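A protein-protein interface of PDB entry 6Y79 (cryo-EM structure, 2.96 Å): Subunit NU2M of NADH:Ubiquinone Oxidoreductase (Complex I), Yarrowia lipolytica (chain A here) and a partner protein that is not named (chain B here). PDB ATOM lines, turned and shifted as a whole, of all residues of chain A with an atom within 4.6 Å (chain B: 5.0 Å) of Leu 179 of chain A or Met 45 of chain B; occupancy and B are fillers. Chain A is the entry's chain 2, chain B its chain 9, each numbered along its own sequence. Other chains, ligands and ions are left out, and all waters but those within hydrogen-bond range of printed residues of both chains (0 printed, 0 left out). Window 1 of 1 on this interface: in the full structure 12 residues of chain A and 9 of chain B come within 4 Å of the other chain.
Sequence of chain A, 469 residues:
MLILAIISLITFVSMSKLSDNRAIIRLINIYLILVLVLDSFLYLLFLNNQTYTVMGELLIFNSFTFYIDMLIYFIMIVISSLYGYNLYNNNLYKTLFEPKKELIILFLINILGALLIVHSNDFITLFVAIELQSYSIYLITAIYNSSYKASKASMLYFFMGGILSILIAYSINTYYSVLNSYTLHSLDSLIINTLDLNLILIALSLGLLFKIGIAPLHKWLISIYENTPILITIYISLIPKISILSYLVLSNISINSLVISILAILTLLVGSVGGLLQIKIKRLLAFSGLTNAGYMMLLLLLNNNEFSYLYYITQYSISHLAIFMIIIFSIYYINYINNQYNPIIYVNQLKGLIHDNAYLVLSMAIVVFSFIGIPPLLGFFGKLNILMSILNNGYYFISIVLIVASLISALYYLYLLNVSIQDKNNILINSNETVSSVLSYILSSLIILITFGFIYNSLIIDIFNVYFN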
ATOM      1  N   TYR A 175      23.282 -23.575   0.264  1.00  0.00           N
ATOM      2  CA  TYR A 175      24.430 -22.675   0.280  1.00  0.00           C
ATOM      3  C   TYR A 175      24.831 -22.274  -1.127  1.00  0.00           C
ATOM      4  O   TYR A 175      25.272 -21.146  -1.352  1.00  0.00           O
ATOM      5  CB  TYR A 175      25.600 -23.358   0.985  1.00  0.00           C
ATOM      6  CG  TYR A 175      26.891 -22.565   1.118  1.00  0.00           C
ATOM      7  CD1 TYR A 175      27.136 -21.780   2.231  1.00  0.00           C
ATOM      8  CD2 TYR A 175      27.888 -22.657   0.158  1.00  0.00           C
ATOM      9  CE1 TYR A 175      28.314 -21.092   2.361  1.00  0.00           C
ATOM     10  CE2 TYR A 175      29.060 -21.976   0.283  1.00  0.00           C
ATOM     11  CZ  TYR A 175      29.271 -21.199   1.379  1.00  0.00           C
ATOM     12  OH  TYR A 175      30.454 -20.521   1.485  1.00  0.00           O
ATOM     13  N   TYR A 176      24.724 -23.203  -2.072  1.00  0.00           N
ATOM     14  CA  TYR A 176      25.076 -22.917  -3.455  1.00  0.00           C
ATOM     15  C   TYR A 176      24.089 -21.960  -4.107  1.00  0.00           C
ATOM     16  O   TYR A 176      24.469 -21.191  -4.994  1.00  0.00           O
ATOM     17  CB  TYR A 176      25.148 -24.225  -4.232  1.00  0.00           C
ATOM     18  CG  TYR A 176      25.443 -24.052  -5.692  1.00  0.00           C
ATOM     19  CD1 TYR A 176      26.715 -23.723  -6.122  1.00  0.00           C
ATOM     20  CD2 TYR A 176      24.449 -24.221  -6.642  1.00  0.00           C
ATOM     21  CE1 TYR A 176      26.986 -23.562  -7.446  1.00  0.00           C
ATOM     22  CE2 TYR A 176      24.709 -24.057  -7.966  1.00  0.00           C
ATOM     23  CZ  TYR A 176      25.974 -23.730  -8.361  1.00  0.00           C
ATOM     24  OH  TYR A 176      26.224 -23.578  -9.692  1.00  0.00           O
ATOM     25  N   SER A 177      22.826 -21.994  -3.682  1.00  0.00           N
ATOM     26  CA  SER A 177      21.798 -21.154  -4.276  1.00  0.00           C
ATOM     27  C   SER A 177      21.946 -19.683  -3.901  1.00  0.00           C
ATOM     28  O   SER A 177      21.362 -18.828  -4.574  1.00  0.00           O
ATOM     29  CB  SER A 177      20.420 -21.657  -3.844  1.00  0.00           C
ATOM     30  OG  SER A 177      20.240 -23.011  -4.160  1.00  0.00           O
ATOM     31  N   VAL A 178      22.677 -19.364  -2.838  1.00  0.00           N
ATOM     32  CA  VAL A 178      22.894 -17.979  -2.450  1.00  0.00           C
ATOM     33  C   VAL A 178      24.310 -17.518  -2.730  1.00  0.00           C
ATOM     34  O   VAL A 178      24.543 -16.306  -2.809  1.00  0.00           O
ATOM     35  CB  VAL A 178      22.534 -17.747  -0.968  1.00  0.00           C
ATOM     36  CG1 VAL A 178      21.128 -18.220  -0.689  1.00  0.00           C
ATOM     37  CG2 VAL A 178      23.500 -18.448  -0.067  1.00  0.00           C
ATOM     38  N   LEU A 179      25.257 -18.428  -2.886  1.00  0.00           N
ATOM     39  CA  LEU A 179      26.629 -18.106  -3.229  1.00  0.00           C
ATOM     40  C   LEU A 179      27.056 -19.081  -4.302  1.00  0.00           C
ATOM     41  O   LEU A 179      27.012 -20.293  -4.086  1.00  0.00           O
ATOM     42  CB  LEU A 179      27.558 -18.235  -2.026  1.00  0.00           C
ATOM     43  CG  LEU A 179      27.443 -17.251  -0.877  1.00  0.00           C
ATOM     44  CD1 LEU A 179      28.375 -17.669   0.229  1.00  0.00           C
ATOM     45  CD2 LEU A 179      27.782 -15.864  -1.366  1.00  0.00           C
ATOM     46  N   ASN A 180      27.494 -18.573  -5.442  1.00  0.00           N
ATOM     47  CA  ASN A 180      28.017 -19.452  -6.478  1.00  0.00           C
ATOM     48  C   ASN A 180      29.411 -19.903  -6.036  1.00  0.00           C
ATOM     49  O   ASN A 180      30.442 -19.403  -6.494  1.00  0.00           O
ATOM     50  CB  ASN A 180      28.018 -18.730  -7.815  1.00  0.00           C
ATOM     51  CG  ASN A 180      28.218 -19.650  -8.967  1.00  0.00           C
ATOM     52  OD1 ASN A 180      28.564 -20.811  -8.790  1.00  0.00           O
ATOM     53  ND2 ASN A 180      28.006 -19.144 -10.169  1.00  0.00           N
ATOM     54  N   SER A 181      29.429 -20.890  -5.139  1.00  0.00           N
ATOM     55  CA  SER A 181      30.654 -21.312  -4.476  1.00  0.00           C
ATOM     56  C   SER A 181      30.422 -22.654  -3.811  1.00  0.00           C
ATOM     57  O   SER A 181      29.286 -23.063  -3.573  1.00  0.00           O
ATOM     58  CB  SER A 181      31.115 -20.287  -3.434  1.00  0.00           C
ATOM     59  OG  SER A 181      32.438 -20.550  -3.016  1.00  0.00           O
ATOM     60  N   SER A 186      35.419 -19.339   0.777  1.00  0.00           N
ATOM     61  CA  SER A 186      34.683 -18.219   0.219  1.00  0.00           C
ATOM     62  C   SER A 186      34.266 -17.188   1.261  1.00  0.00           C
ATOM     63  O   SER A 186      34.091 -16.024   0.900  1.00  0.00           O
ATOM     64  CB  SER A 186      33.442 -18.726  -0.501  1.00  0.00           C
ATOM     65  OG  SER A 186      32.421 -17.754  -0.483  1.00  0.00           O
ATOM     66  N   LEU A 187      34.122 -17.572   2.534  1.00  0.00           N
ATOM     67  CA  LEU A 187      33.419 -16.741   3.510  1.00  0.00           C
ATOM     68  C   LEU A 187      34.209 -15.488   3.891  1.00  0.00           C
ATOM     69  O   LEU A 187      33.636 -14.397   3.958  1.00  0.00           O
ATOM     70  CB  LEU A 187      33.092 -17.571   4.748  1.00  0.00           C
ATOM     71  CG  LEU A 187      32.061 -18.675   4.541  1.00  0.00           C
ATOM     72  CD1 LEU A 187      31.687 -19.324   5.862  1.00  0.00           C
ATOM     73  CD2 LEU A 187      30.840 -18.128   3.862  1.00  0.00           C
ATOM     74  N   LEU A 195      25.468 -10.985   5.019  1.00  0.00           N
ATOM     75  CA  LEU A 195      24.669 -12.074   4.471  1.00  0.00           C
ATOM     76  C   LEU A 195      24.173 -12.941   5.619  1.00  0.00           C
ATOM     77  O   LEU A 195      24.935 -13.242   6.541  1.00  0.00           O
ATOM     78  CB  LEU A 195      25.493 -12.915   3.493  1.00  0.00           C
ATOM     79  CG  LEU A 195      24.857 -13.747   2.396  1.00  0.00           C
ATOM     80  CD1 LEU A 195      24.178 -12.822   1.454  1.00  0.00           C
ATOM     81  CD2 LEU A 195      25.917 -14.544   1.667  1.00  0.00           C
ATOM     82  N   LEU A 197      23.863 -16.152   6.478  1.00  0.00           N
ATOM     83  CA  LEU A 197      24.238 -17.541   6.291  1.00  0.00           C
ATOM     84  C   LEU A 197      23.997 -18.367   7.538  1.00  0.00           C
ATOM     85  O   LEU A 197      24.442 -19.512   7.596  1.00  0.00           O
ATOM     86  CB  LEU A 197      25.698 -17.642   5.868  1.00  0.00           C
ATOM     87  CG  LEU A 197      25.951 -17.038   4.496  1.00  0.00           C
ATOM     88  CD1 LEU A 197      27.422 -16.824   4.307  1.00  0.00           C
ATOM     89  CD2 LEU A 197      25.397 -17.939   3.421  1.00  0.00           C
ATOM     90  N   PHE B  41      31.260  -6.829  -3.526  1.00  0.00           N
ATOM     91  CA  PHE B  41      30.445  -7.945  -3.061  1.00  0.00           C
ATOM     92  C   PHE B  41      28.969  -7.709  -3.326  1.00  0.00           C
ATOM     93  O   PHE B  41      28.275  -8.622  -3.792  1.00  0.00           O
ATOM     94  CB  PHE B  41      30.659  -8.186  -1.573  1.00  0.00           C
ATOM     95  CG  PHE B  41      29.879  -9.341  -1.048  1.00  0.00           C
ATOM     96  CD1 PHE B  41      30.189 -10.627  -1.442  1.00  0.00           C
ATOM     97  CD2 PHE B  41      28.819  -9.144  -0.184  1.00  0.00           C
ATOM     98  CE1 PHE B  41      29.468 -11.695  -0.975  1.00  0.00           C
ATOM     99  CE2 PHE B  41      28.098 -10.212   0.289  1.00  0.00           C
ATOM    100  CZ  PHE B  41      28.430 -11.489  -0.101  1.00  0.00           C
ATOM    101  N   GLU B  42      28.494  -6.479  -3.085  1.00  0.00           N
ATOM    102  CA  GLU B  42      27.108  -6.146  -3.390  1.00  0.00           C
ATOM    103  C   GLU B  42      26.843  -6.294  -4.877  1.00  0.00           C
ATOM    104  O   GLU B  42      25.860  -6.938  -5.272  1.00  0.00           O
ATOM    105  CB  GLU B  42      26.791  -4.730  -2.921  1.00  0.00           C
ATOM    106  CG  GLU B  42      26.626  -4.589  -1.423  1.00  0.00           C
ATOM    107  CD  GLU B  42      26.521  -3.142  -0.985  1.00  0.00           C
ATOM    108  OE1 GLU B  42      26.675  -2.250  -1.844  1.00  0.00           O
ATOM    109  OE2 GLU B  42      26.289  -2.896   0.217  1.00  0.00           O
ATOM    110  N   ASP B  43      27.794  -5.826  -5.698  1.00  0.00           N
ATOM    111  CA  ASP B  43      27.703  -5.976  -7.146  1.00  0.00           C
ATOM    112  C   ASP B  43      27.693  -7.435  -7.549  1.00  0.00           C
ATOM    113  O   ASP B  43      27.062  -7.807  -8.542  1.00  0.00           O
ATOM    114  CB  ASP B  43      28.873  -5.274  -7.822  1.00  0.00           C
ATOM    115  CG  ASP B  43      28.809  -3.792  -7.669  1.00  0.00           C
ATOM    116  OD1 ASP B  43      27.741  -3.309  -7.249  1.00  0.00           O
ATOM    117  OD2 ASP B  43      29.815  -3.116  -7.966  1.00  0.00           O
ATOM    118  N   TYR B  44      28.377  -8.279  -6.781  1.00  0.00           N
ATOM    119  CA  TYR B  44      28.348  -9.694  -7.090  1.00  0.00           C
ATOM    120  C   TYR B  44      27.004 -10.292  -6.727  1.00  0.00           C
ATOM    121  O   TYR B  44      26.420 -11.035  -7.525  1.00  0.00           O
ATOM    122  CB  TYR B  44      29.465 -10.417  -6.361  1.00  0.00           C
ATOM    123  CG  TYR B  44      29.489 -11.871  -6.695  1.00  0.00           C
ATOM    124  CD1 TYR B  44      29.650 -12.286  -8.003  1.00  0.00           C
ATOM    125  CD2 TYR B  44      29.331 -12.835  -5.713  1.00  0.00           C
ATOM    126  CE1 TYR B  44      29.661 -13.612  -8.325  1.00  0.00           C
ATOM    127  CE2 TYR B  44      29.344 -14.166  -6.029  1.00  0.00           C
ATOM    128  CZ  TYR B  44      29.513 -14.546  -7.338  1.00  0.00           C
ATOM    129  OH  TYR B  44      29.536 -15.870  -7.675  1.00  0.00           O
ATOM    130  N   MET B  45      26.471  -9.926  -5.557  1.00  0.00           N
ATOM    131  CA  MET B  45      25.314 -10.642  -5.032  1.00  0.00           C
ATOM    132  C   MET B  45      24.075 -10.330  -5.836  1.00  0.00           C
ATOM    133  O   MET B  45      23.311 -11.230  -6.202  1.00  0.00           O
ATOM    134  CB  MET B  45      25.086 -10.292  -3.570  1.00  0.00           C
ATOM    135  CG  MET B  45      26.094 -10.907  -2.667  1.00  0.00           C
ATOM    136  SD  MET B  45      26.148 -12.690  -2.850  1.00  0.00           S
ATOM    137  CE  MET B  45      24.509 -13.080  -2.273  1.00  0.00           C
ATOM    138  N   GLU B  46      23.900  -9.074  -6.189  1.00  0.00           N
ATOM    139  CA  GLU B  46      22.781  -8.756  -7.042  1.00  0.00           C
ATOM    140  C   GLU B  46      23.066  -9.086  -8.510  1.00  0.00           C
ATOM    141  O   GLU B  46      22.120  -9.169  -9.293  1.00  0.00           O
ATOM    142  CB  GLU B  46      22.374  -7.305  -6.765  1.00  0.00           C
ATOM    143  CG  GLU B  46      21.098  -6.868  -7.355  1.00  0.00           C
ATOM    144  CD  GLU B  46      21.370  -6.203  -8.678  1.00  0.00           C
ATOM    145  OE1 GLU B  46      22.402  -5.514  -8.712  1.00  0.00           O
ATOM    146  OE2 GLU B  46      20.602  -6.387  -9.609  1.00  0.00           O
ATOM    147  N   CYS B  47      24.324  -9.371  -8.890  1.00  0.00           N
ATOM    148  CA  CYS B  47      24.541 -10.090 -10.144  1.00  0.00           C
ATOM    149  C   CYS B  47      23.887 -11.454 -10.090  1.00  0.00           C
ATOM    150  O   CYS B  47      23.307 -11.910 -11.078  1.00  0.00           O
ATOM    151  CB  CYS B  47      26.026 -10.270 -10.450  1.00  0.00           C
ATOM    152  SG  CYS B  47      26.377 -11.146 -12.035  1.00  0.00           S
ATOM    153  N   LEU B  48      23.990 -12.127  -8.945  1.00  0.00           N
ATOM    154  CA  LEU B  48      23.469 -13.478  -8.821  1.00  0.00           C
ATOM    155  C   LEU B  48      21.951 -13.481  -8.829  1.00  0.00           C
ATOM    156  O   LEU B  48      21.320 -14.218  -9.592  1.00  0.00           O
ATOM    157  CB  LEU B  48      23.990 -14.113  -7.536  1.00  0.00           C
ATOM    158  CG  LEU B  48      25.466 -14.449  -7.436  1.00  0.00           C
ATOM    159  CD1 LEU B  48      25.752 -14.944  -6.042  1.00  0.00           C
ATOM    160  CD2 LEU B  48      25.826 -15.490  -8.462  1.00  0.00           C
ATOM    161  N   HIS B  49      21.346 -12.645  -7.992  1.00  0.00           N
ATOM    162  CA  HIS B  49      19.945 -12.805  -7.654  1.00  0.00           C
ATOM    163  C   HIS B  49      19.040 -11.708  -8.181  1.00  0.00           C
ATOM    164  O   HIS B  49      17.820 -11.885  -8.128  1.00  0.00           O
ATOM    165  CB  HIS B  49      19.791 -12.905  -6.134  1.00  0.00           C
ATOM    166  CG  HIS B  49      20.466 -14.103  -5.551  1.00  0.00           C
ATOM    167  ND1 HIS B  49      21.713 -14.047  -4.976  1.00  0.00           N
ATOM    168  CD2 HIS B  49      20.078 -15.398  -5.488  1.00  0.00           C
ATOM    169  CE1 HIS B  49      22.059 -15.252  -4.565  1.00  0.00           C
ATOM    170  NE2 HIS B  49      21.084 -16.090  -4.863  1.00  0.00           N
ATOM    171  N   HIS B  50      19.606 -10.600  -8.682  1.00  0.00           N
ATOM    172  CA  HIS B  50      18.866  -9.488  -9.296  1.00  0.00           C
ATOM    173  C   HIS B  50      17.843  -8.886  -8.337  1.00  0.00           C
ATOM    174  O   HIS B  50      16.697  -8.640  -8.704  1.00  0.00           O
ATOM    175  CB  HIS B  50      18.197  -9.908 -10.607  1.00  0.00           C
ATOM    176  CG  HIS B  50      19.155 -10.335 -11.671  1.00  0.00           C
ATOM    177  ND1 HIS B  50      20.049  -9.468 -12.258  1.00  0.00           N
ATOM    178  CD2 HIS B  50      19.343 -11.533 -12.269  1.00  0.00           C
ATOM    179  CE1 HIS B  50      20.757 -10.118 -13.163  1.00  0.00           C
ATOM    180  NE2 HIS B  50      20.349 -11.372 -13.190  1.00  0.00           N
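The backbone carbonyl oxygen (O) of Met 45 of chain B lies within hydrogen-bond range of a ring nitrogen (ND1) of His 49 of chain B, 3.5 Å away.
Of chain B, only Met 45 comes within 4 Å of Leu 179 of chain A.
Of the printed residues of chain A, Met 45 of chain B touches Val 178 (3.3 Å), Leu 179 (3.9 Å) and Leu 195 (3.8 Å).
Of the printed residues of chain A, Tyr 44 of chain B touches Asn 180 (3.2 Å).
Of the printed residues of chain A, Leu 48 of chain B touches Val 178 and Asn 180.
Printed residues of chain B within 4 Å of Asn 180 of chain A: Tyr 44 (3.2 Å) and Leu 48 (3.96 Å).
Ser 181 of chain A touches none of the printed residues of chain B.
Among the printed residues, merely in contact across the chains: Val 178 of chain A with His 49 of chain B, Asn 180 of chain A with Tyr 44 of chain B, Val 178 of chain A with Met 45 of chain B, Val 178 of chain A with Leu 48 of chain B, Leu 195 of chain A with Met 45 of chain B, Leu 179 of chain A with Met 45 of chain B and Asn 180 of chain A with Leu 48 of chain B.
NE2 of His 49 of chain B lies within hydrogen-bond range of O of Ser 177 of chain A, 2.8 Å away.
Printed residues of chain A that touch a printed residue of chain B: Ser 177, Val 178, Leu 179, Asn 180 and Leu 195.
Of the 10 printed residues of chain B, 4 touch a printed residue of chain A.
Hydrophobic or aromatic side chains of chain B that line the printed part of chain A: Tyr 44, Met 45, Leu 48 and His 49.
Among the printed residues, no Asp or Glu carboxylate lies within 4 Å of a Lys or Arg side-chain nitrogen of the other chain.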
